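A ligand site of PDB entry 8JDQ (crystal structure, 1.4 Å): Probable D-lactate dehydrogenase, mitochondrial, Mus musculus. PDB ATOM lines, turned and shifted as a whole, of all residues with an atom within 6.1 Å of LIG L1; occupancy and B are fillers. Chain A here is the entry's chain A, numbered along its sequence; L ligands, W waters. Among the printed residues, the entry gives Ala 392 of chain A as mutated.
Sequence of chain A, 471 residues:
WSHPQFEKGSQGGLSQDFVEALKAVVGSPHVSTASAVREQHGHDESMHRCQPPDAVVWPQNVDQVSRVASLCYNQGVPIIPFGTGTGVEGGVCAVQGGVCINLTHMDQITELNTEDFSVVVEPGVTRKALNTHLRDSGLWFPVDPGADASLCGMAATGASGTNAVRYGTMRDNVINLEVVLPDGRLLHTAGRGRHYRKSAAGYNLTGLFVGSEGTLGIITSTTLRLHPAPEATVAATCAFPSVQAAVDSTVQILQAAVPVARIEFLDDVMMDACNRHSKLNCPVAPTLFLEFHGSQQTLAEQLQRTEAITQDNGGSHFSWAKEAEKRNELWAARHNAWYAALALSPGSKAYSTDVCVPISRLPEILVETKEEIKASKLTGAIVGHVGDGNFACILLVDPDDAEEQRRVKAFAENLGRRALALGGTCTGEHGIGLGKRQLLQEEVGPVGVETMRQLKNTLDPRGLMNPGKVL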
ATOM      1  N   VAL A  88      18.482 -25.211  18.975  1.00  0.00           N
ATOM      2  CA  VAL A  88      19.729 -25.297  19.733  1.00  0.00           C
ATOM      3  C   VAL A  88      19.764 -26.509  20.666  1.00  0.00           C
ATOM      4  O   VAL A  88      20.608 -26.567  21.556  1.00  0.00           O
ATOM      5  CB  VAL A  88      20.055 -23.980  20.478  1.00  0.00           C
ATOM      6  CG1 VAL A  88      20.180 -22.826  19.492  1.00  0.00           C
ATOM      7  CG2 VAL A  88      18.985 -23.687  21.532  1.00  0.00           C
ATOM      8  N   GLY A 146      16.148 -14.511  17.557  1.00  0.00           N
ATOM      9  CA  GLY A 146      17.204 -13.842  16.816  1.00  0.00           C
ATOM     10  C   GLY A 146      17.437 -14.403  15.423  1.00  0.00           C
ATOM     11  O   GLY A 146      17.878 -13.690  14.526  1.00  0.00           O
ATOM     12  N   GLU A 264      16.341  -6.545  27.887  1.00  0.00           N
ATOM     13  CA  GLU A 264      17.294  -7.592  27.569  1.00  0.00           C
ATOM     14  C   GLU A 264      18.597  -7.338  28.307  1.00  0.00           C
ATOM     15  O   GLU A 264      19.085  -6.199  28.347  1.00  0.00           O
ATOM     16  CB  GLU A 264      17.558  -7.613  26.066  1.00  0.00           C
ATOM     17  CG  GLU A 264      16.372  -8.111  25.256  1.00  0.00           C
ATOM     18  CD  GLU A 264      16.104  -9.587  25.474  1.00  0.00           C
ATOM     19  OE1 GLU A 264      17.079 -10.360  25.482  1.00  0.00           O
ATOM     20  OE2 GLU A 264      14.928  -9.969  25.619  1.00  0.00           O
ATOM     21  N   ARG A 334      21.640  -7.456  19.142  1.00  0.00           N
ATOM     22  CA  ARG A 334      21.105  -8.362  20.149  1.00  0.00           C
ATOM     23  C   ARG A 334      20.699  -9.683  19.529  1.00  0.00           C
ATOM     24  O   ARG A 334      21.053 -10.753  20.034  1.00  0.00           O
ATOM     25  CB  ARG A 334      19.914  -7.712  20.859  1.00  0.00           C
ATOM     26  CG  ARG A 334      19.093  -8.676  21.706  1.00  0.00           C
ATOM     27  CD  ARG A 334      19.896  -9.255  22.872  1.00  0.00           C
ATOM     28  NE  ARG A 334      19.111 -10.262  23.587  1.00  0.00           N
ATOM     29  CZ  ARG A 334      19.083 -11.552  23.261  1.00  0.00           C
ATOM     30  NH1 ARG A 334      19.817 -12.017  22.259  1.00  0.00           N
ATOM     31  NH2 ARG A 334      18.315 -12.388  23.959  1.00  0.00           N
ATOM     32  N   HIS A 335      19.957  -9.635  18.417  1.00  0.00           N
ATOM     33  CA  HIS A 335      19.491 -10.859  17.775  1.00  0.00           C
ATOM     34  C   HIS A 335      20.647 -11.761  17.344  1.00  0.00           C
ATOM     35  O   HIS A 335      20.502 -12.986  17.320  1.00  0.00           O
ATOM     36  CB  HIS A 335      18.609 -10.523  16.581  1.00  0.00           C
ATOM     37  CG  HIS A 335      17.225 -10.094  16.957  1.00  0.00           C
ATOM     38  ND1 HIS A 335      16.499  -9.173  16.237  1.00  0.00           N
ATOM     39  CD2 HIS A 335      16.413 -10.499  17.966  1.00  0.00           C
ATOM     40  CE1 HIS A 335      15.314  -9.013  16.790  1.00  0.00           C
ATOM     41  NE2 HIS A 335      15.231  -9.804  17.843  1.00  0.00           N
ATOM     42  N   ALA A 337      23.522 -12.107  18.952  1.00  0.00           N
ATOM     43  CA  ALA A 337      24.407 -12.368  20.081  1.00  0.00           C
ATOM     44  C   ALA A 337      25.040 -13.754  20.011  1.00  0.00           C
ATOM     45  O   ALA A 337      26.232 -13.921  20.312  1.00  0.00           O
ATOM     46  CB  ALA A 337      23.618 -12.224  21.389  1.00  0.00           C
ATOM     47  N   TRP A 338      24.264 -14.765  19.624  1.00  0.00           N
ATOM     48  CA  TRP A 338      24.801 -16.117  19.462  1.00  0.00           C
ATOM     49  C   TRP A 338      26.036 -16.113  18.559  1.00  0.00           C
ATOM     50  O   TRP A 338      27.084 -16.656  18.912  1.00  0.00           O
ATOM     51  CB  TRP A 338      23.712 -17.011  18.874  1.00  0.00           C
ATOM     52  CG  TRP A 338      24.105 -18.406  18.488  1.00  0.00           C
ATOM     53  CD1 TRP A 338      24.190 -18.905  17.217  1.00  0.00           C
ATOM     54  CD2 TRP A 338      24.402 -19.501  19.367  1.00  0.00           C
ATOM     55  NE1 TRP A 338      24.539 -20.229  17.252  1.00  0.00           N
ATOM     56  CE2 TRP A 338      24.685 -20.623  18.556  1.00  0.00           C
ATOM     57  CE3 TRP A 338      24.476 -19.635  20.758  1.00  0.00           C
ATOM     58  CZ2 TRP A 338      25.024 -21.865  19.089  1.00  0.00           C
ATOM     59  CZ3 TRP A 338      24.823 -20.876  21.280  1.00  0.00           C
ATOM     60  CH2 TRP A 338      25.084 -21.976  20.454  1.00  0.00           C
ATOM     61  N   SER A 352      24.495 -24.126  25.198  1.00  0.00           N
ATOM     62  CA  SER A 352      23.616 -23.079  25.707  1.00  0.00           C
ATOM     63  C   SER A 352      22.854 -23.594  26.921  1.00  0.00           C
ATOM     64  O   SER A 352      22.702 -24.796  27.133  1.00  0.00           O
ATOM     65  CB  SER A 352      22.611 -22.625  24.646  1.00  0.00           C
ATOM     66  OG  SER A 352      21.745 -23.692  24.280  1.00  0.00           O
ATOM     67  N   THR A 353      22.399 -22.651  27.735  1.00  0.00           N
ATOM     68  CA  THR A 353      21.408 -22.904  28.777  1.00  0.00           C
ATOM     69  C   THR A 353      20.243 -21.951  28.552  1.00  0.00           C
ATOM     70  O   THR A 353      20.319 -21.046  27.715  1.00  0.00           O
ATOM     71  CB  THR A 353      22.012 -22.694  30.180  1.00  0.00           C
ATOM     72  OG1 THR A 353      22.381 -21.325  30.342  1.00  0.00           O
ATOM     73  CG2 THR A 353      23.236 -23.579  30.370  1.00  0.00           C
ATOM     74  N   ASP A 354      19.165 -22.136  29.310  1.00  0.00           N
ATOM     75  CA  ASP A 354      17.936 -21.415  29.024  1.00  0.00           C
ATOM     76  C   ASP A 354      17.007 -21.435  30.230  1.00  0.00           C
ATOM     77  O   ASP A 354      15.787 -21.498  30.075  1.00  0.00           O
ATOM     78  CB  ASP A 354      17.240 -22.077  27.820  1.00  0.00           C
ATOM     79  CG  ASP A 354      16.018 -21.310  27.334  1.00  0.00           C
ATOM     80  OD1 ASP A 354      15.991 -20.058  27.421  1.00  0.00           O
ATOM     81  OD2 ASP A 354      15.066 -21.982  26.875  1.00  0.00           O
ATOM     82  N   VAL A 383      23.340 -13.648  28.142  1.00  0.00           N
ATOM     83  CA  VAL A 383      22.377 -12.785  27.477  1.00  0.00           C
ATOM     84  C   VAL A 383      21.000 -13.302  27.849  1.00  0.00           C
ATOM     85  O   VAL A 383      20.822 -14.494  28.087  1.00  0.00           O
ATOM     86  CB  VAL A 383      22.609 -12.763  25.953  1.00  0.00           C
ATOM     87  CG1 VAL A 383      22.211 -14.104  25.330  1.00  0.00           C
ATOM     88  CG2 VAL A 383      21.859 -11.614  25.309  1.00  0.00           C
ATOM     89  N   GLY A 384      20.019 -12.406  27.944  1.00  0.00           N
ATOM     90  CA  GLY A 384      18.762 -12.965  28.372  1.00  0.00           C
ATOM     91  C   GLY A 384      17.509 -12.120  28.326  1.00  0.00           C
ATOM     92  O   GLY A 384      17.552 -10.903  28.530  1.00  0.00           O
ATOM     93  N   HIS A 385      16.384 -12.809  28.099  1.00  0.00           N
ATOM     94  CA  HIS A 385      15.032 -12.261  28.216  1.00  0.00           C
ATOM     95  C   HIS A 385      14.679 -12.172  29.710  1.00  0.00           C
ATOM     96  O   HIS A 385      13.784 -12.854  30.218  1.00  0.00           O
ATOM     97  CB  HIS A 385      14.043 -13.172  27.508  1.00  0.00           C
ATOM     98  CG  HIS A 385      14.438 -13.553  26.113  1.00  0.00           C
ATOM     99  ND1 HIS A 385      14.769 -12.616  25.153  1.00  0.00           N
ATOM    100  CD2 HIS A 385      14.539 -14.760  25.508  1.00  0.00           C
ATOM    101  CE1 HIS A 385      15.045 -13.231  24.022  1.00  0.00           C
ATOM    102  NE2 HIS A 385      14.912 -14.532  24.202  1.00  0.00           N
ATOM    103  N   ALA A 392      20.150 -16.955  29.039  1.00  0.00           N
ATOM    104  CA  ALA A 392      20.956 -17.976  28.392  1.00  0.00           C
ATOM    105  C   ALA A 392      22.426 -17.751  28.702  1.00  0.00           C
ATOM    106  O   ALA A 392      22.912 -16.617  28.680  1.00  0.00           O
ATOM    107  CB  ALA A 392      20.763 -17.955  26.879  1.00  0.00           C
ATOM    108  N   CYS A 393      23.118 -18.838  28.995  1.00  0.00           N
ATOM    109  CA  CYS A 393      24.569 -18.878  28.989  1.00  0.00           C
ATOM    110  C   CYS A 393      24.993 -19.415  27.636  1.00  0.00           C
ATOM    111  O   CYS A 393      24.459 -20.428  27.177  1.00  0.00           O
ATOM    112  CB  CYS A 393      25.054 -19.859  30.040  1.00  0.00           C
ATOM    113  SG  CYS A 393      24.979 -19.238  31.677  1.00  0.00           S
ATOM    114  N   ILE A 394      25.957 -18.760  27.011  1.00  0.00           N
ATOM    115  CA  ILE A 394      26.547 -19.247  25.777  1.00  0.00           C
ATOM    116  C   ILE A 394      27.955 -19.704  26.127  1.00  0.00           C
ATOM    117  O   ILE A 394      28.793 -18.889  26.526  1.00  0.00           O
ATOM    118  CB  ILE A 394      26.545 -18.185  24.671  1.00  0.00           C
ATOM    119  CG1 ILE A 394      25.097 -17.798  24.352  1.00  0.00           C
ATOM    120  CG2 ILE A 394      27.242 -18.709  23.426  1.00  0.00           C
ATOM    121  CD1 ILE A 394      24.953 -16.537  23.533  1.00  0.00           C
ATOM    122  N   GLU A 429      12.348 -21.312  26.645  1.00  0.00           N
ATOM    123  CA  GLU A 429      11.921 -21.143  25.256  1.00  0.00           C
ATOM    124  C   GLU A 429      12.546 -22.135  24.266  1.00  0.00           C
ATOM    125  O   GLU A 429      11.896 -22.495  23.285  1.00  0.00           O
ATOM    126  CB  GLU A 429      12.185 -19.698  24.792  1.00  0.00           C
ATOM    127  CG  GLU A 429      13.638 -19.237  24.932  1.00  0.00           C
ATOM    128  CD  GLU A 429      13.918 -17.879  24.294  1.00  0.00           C
ATOM    129  OE1 GLU A 429      12.960 -17.187  23.888  1.00  0.00           O
ATOM    130  OE2 GLU A 429      15.109 -17.511  24.185  1.00  0.00           O
ATOM    131  N   HIS A 430      13.781 -22.581  24.494  1.00  0.00           N
ATOM    132  CA  HIS A 430      14.494 -23.375  23.476  1.00  0.00           C
ATOM    133  C   HIS A 430      13.933 -24.773  23.334  1.00  0.00           C
ATOM    134  O   HIS A 430      13.994 -25.355  22.242  1.00  0.00           O
ATOM    135  CB  HIS A 430      15.962 -23.485  23.827  1.00  0.00           C
ATOM    136  CG  HIS A 430      16.688 -22.184  23.780  1.00  0.00           C
ATOM    137  ND1 HIS A 430      17.851 -21.969  24.487  1.00  0.00           N
ATOM    138  CD2 HIS A 430      16.429 -21.047  23.102  1.00  0.00           C
ATOM    139  CE1 HIS A 430      18.267 -20.734  24.263  1.00  0.00           C
ATOM    140  NE2 HIS A 430      17.429 -20.157  23.419  1.00  0.00           N
HETATM  141  C1  LIG L   1      18.922 -16.971  21.986  1.00  0.00           C
HETATM  142  O1  LIG L   1      18.050 -15.018  23.115  1.00  0.00           O
HETATM  143  C2  LIG L   1      20.257 -17.488  22.516  1.00  0.00           C
HETATM  144  O2  LIG L   1      19.474 -14.669  21.498  1.00  0.00           O
HETATM  145  C3  LIG L   1      18.812 -15.463  22.212  1.00  0.00           C
HETATM  146  O3  LIG L   1      17.862 -17.612  22.638  1.00  0.00           O
HETATM  147  C4  LIG L   1      20.448 -18.932  22.038  1.00  0.00           C
HETATM  148  C5  LIG L   1      20.904 -18.981  20.591  1.00  0.00           C
HETATM  149  C6  LIG L   1      21.468 -19.645  22.920  1.00  0.00           C
HETATM  150  P1  LG2 L   2      14.347 -26.617  13.646  1.00  0.00           P
HETATM  151  O1  LG2 L   2      15.731 -26.635  14.183  1.00  0.00           O
HETATM  152  O2  LG2 L   2      14.133 -26.878  12.162  1.00  0.00           O
HETATM  153  O3  LG2 L   2      13.477 -27.646  14.465  1.00  0.00           O
HETATM  154  C1  LG2 L   2      13.330 -27.497  15.899  1.00  0.00           C
HETATM  155  C2  LG2 L   2      12.482 -28.608  16.463  1.00  0.00           C
HETATM  156  O4  LG2 L   2      11.113 -28.422  16.071  1.00  0.00           O
HETATM  157  C3  LG2 L   2      12.859 -30.015  15.987  1.00  0.00           C
HETATM  158  O5  LG2 L   2      12.599 -30.972  17.014  1.00  0.00           O
HETATM  159  C4  LG2 L   2      11.972 -30.199  14.756  1.00  0.00           C
HETATM  160  O6  LG2 L   2      11.678 -31.566  14.500  1.00  0.00           O
HETATM  161  C5  LG2 L   2      10.706 -29.450  15.182  1.00  0.00           C
HETATM  162  N1  LG2 L   2       9.959 -28.840  14.092  1.00  0.00           N
HETATM  163  C6  LG2 L   2      10.372 -27.856  13.234  1.00  0.00           C
HETATM  164  N2  LG2 L   2       9.452 -27.465  12.387  1.00  0.00           N
HETATM  165  C7  LG2 L   2       8.351 -28.229  12.730  1.00  0.00           C
HETATM  166  C8  LG2 L   2       7.045 -28.298  12.203  1.00  0.00           C
HETATM  167  N3  LG2 L   2       6.598 -27.535  11.207  1.00  0.00           N
HETATM  168  N4  LG2 L   2       6.191 -29.178  12.778  1.00  0.00           N
HETATM  169  C9  LG2 L   2       6.623 -29.932  13.798  1.00  0.00           C
HETATM  170  N5  LG2 L   2       7.820 -29.949  14.366  1.00  0.00           N
HETATM  171  C10 LG2 L   2       8.651 -29.077  13.784  1.00  0.00           C
HETATM  172  N6  LG2 L   2      14.641 -19.513  20.245  1.00  0.00           N
HETATM  173  C11 LG2 L   2      13.796 -18.845  21.071  1.00  0.00           C
HETATM  174  O7  LG2 L   2      12.807 -19.399  21.576  1.00  0.00           O
HETATM  175  N7  LG2 L   2      14.010 -17.503  21.338  1.00  0.00           N
HETATM  176  C12 LG2 L   2      15.036 -16.733  20.856  1.00  0.00           C
HETATM  177  O8  LG2 L   2      15.139 -15.548  21.180  1.00  0.00           O
HETATM  178  C13 LG2 L   2      15.938 -17.450  19.966  1.00  0.00           C
HETATM  179  N8  LG2 L   2      16.940 -16.784  19.438  1.00  0.00           N
HETATM  180  C14 LG2 L   2      17.792 -17.472  18.599  1.00  0.00           C
HETATM  181  C15 LG2 L   2      18.870 -16.789  18.039  1.00  0.00           C
HETATM  182  C16 LG2 L   2      19.761 -17.427  17.178  1.00  0.00           C
HETATM  183  C17 LG2 L   2      20.913 -16.647  16.594  1.00  0.00           C
HETATM  184  C18 LG2 L   2      19.582 -18.789  16.882  1.00  0.00           C
HETATM  185  C19 LG2 L   2      20.530 -19.507  15.963  1.00  0.00           C
HETATM  186  C20 LG2 L   2      18.504 -19.472  17.442  1.00  0.00           C
HETATM  187  C21 LG2 L   2      17.622 -18.834  18.301  1.00  0.00           C
HETATM  188  N9  LG2 L   2      16.515 -19.505  18.867  1.00  0.00           N
HETATM  189  C22 LG2 L   2      15.654 -18.838  19.716  1.00  0.00           C
HETATM  190  C23 LG2 L   2      16.303 -20.941  18.642  1.00  0.00           C
HETATM  191  C24 LG2 L   2      15.504 -21.279  17.383  1.00  0.00           C
HETATM  192  O9  LG2 L   2      15.598 -20.235  16.422  1.00  0.00           O
HETATM  193  C25 LG2 L   2      14.054 -21.520  17.771  1.00  0.00           C
HETATM  194  O10 LG2 L   2      13.993 -22.640  18.648  1.00  0.00           O
HETATM  195  C26 LG2 L   2      13.147 -21.754  16.560  1.00  0.00           C
HETATM  196  O11 LG2 L   2      11.796 -21.856  17.005  1.00  0.00           O
HETATM  197  C27 LG2 L   2      13.532 -23.008  15.791  1.00  0.00           C
HETATM  198  O12 LG2 L   2      12.803 -23.030  14.538  1.00  0.00           O
HETATM  199  P2  LG2 L   2      13.347 -23.878  13.330  1.00  0.00           P
HETATM  200  O13 LG2 L   2      12.266 -24.052  12.267  1.00  0.00           O
HETATM  201  O14 LG2 L   2      14.637 -23.297  12.847  1.00  0.00           O
HETATM  202  O15 LG2 L   2      13.610 -25.271  14.056  1.00  0.00           O
HETATM  203  O   HOH W   1      17.750 -13.021  19.842  1.00  0.00           O
HETATM  204  O   HOH W   2      21.447 -14.579  19.500  1.00  0.00           O
HETATM  205  O   HOH W   3      18.411 -15.888  25.684  1.00  0.00           O
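O3 of LIG L1 lies close to N8 of LG2 L2 (3.4 Å).
CE3 of Trp 338 touches C5 of LIG L1, at 3.6 Å.
Ser 352 touches LIG L1 (CB to C6, 3.6 Å).
Six residues have an atom within 4 Å of LIG L1: Arg 334, Trp 338, Ser 352, His 385, Glu 429 and His 430.
The nearest printed residue that does not touch LIG L1 is Val 88 (4.1 Å).
OD2 of Asp 354 lies within hydrogen-bond range of N of His 430, 2.8 Å away.
The guanidinium group (NE) of Arg 334 is in salt-bridge range of the side-chain carboxylate (OE1) of Glu 264 (2.8 Å).
NE2 of His 385 is in hydrogen-bond range of OE2 of Glu 429.
OD2 of Asp 354 sits at hydrogen-bond distance from N of Glu 429, 2.8 Å away.
A ring nitrogen (ND1) of His 385 is in hydrogen-bond range of the side-chain carboxylate of Glu 264, 2.7 Å away.
A ring nitrogen (NE2) of His 430 is in hydrogen-bond range of an oxygen (O3) of LIG L1.
NH2 of Arg 334 lies within salt-bridge range of O1 of LIG L1, at 2.8 Å.
An oxygen (O3) of LIG L1 is in hydrogen-bond range of the side-chain carboxylate (OE2) of Glu 429 (3.2 Å).
A ring nitrogen (NE2) of His 385 lies within hydrogen-bond range of an oxygen (O1) of LIG L1, at 3.4 Å.
A nitrogen (N7) of LG2 L2 sits at hydrogen-bond distance from the side-chain carboxylate of Glu 429.
NE2 of His 385 lies within hydrogen-bond range of O8 of LG2 L2 (3.2 Å).
N of Gly 146 is in hydrogen-bond range of N8 of LG2 L2 (3.1 Å).
Water W2 lies within hydrogen-bond range of O2 of LIG L1 (2.8 Å), N of Trp 338 (2.8 Å), O of His 335 (2.9 Å) and N of Ala 337 (3.3 Å).
Water W1 lies within hydrogen-bond range of O2 of LIG L1, N of Gly 146 and NH1 of Arg 334.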
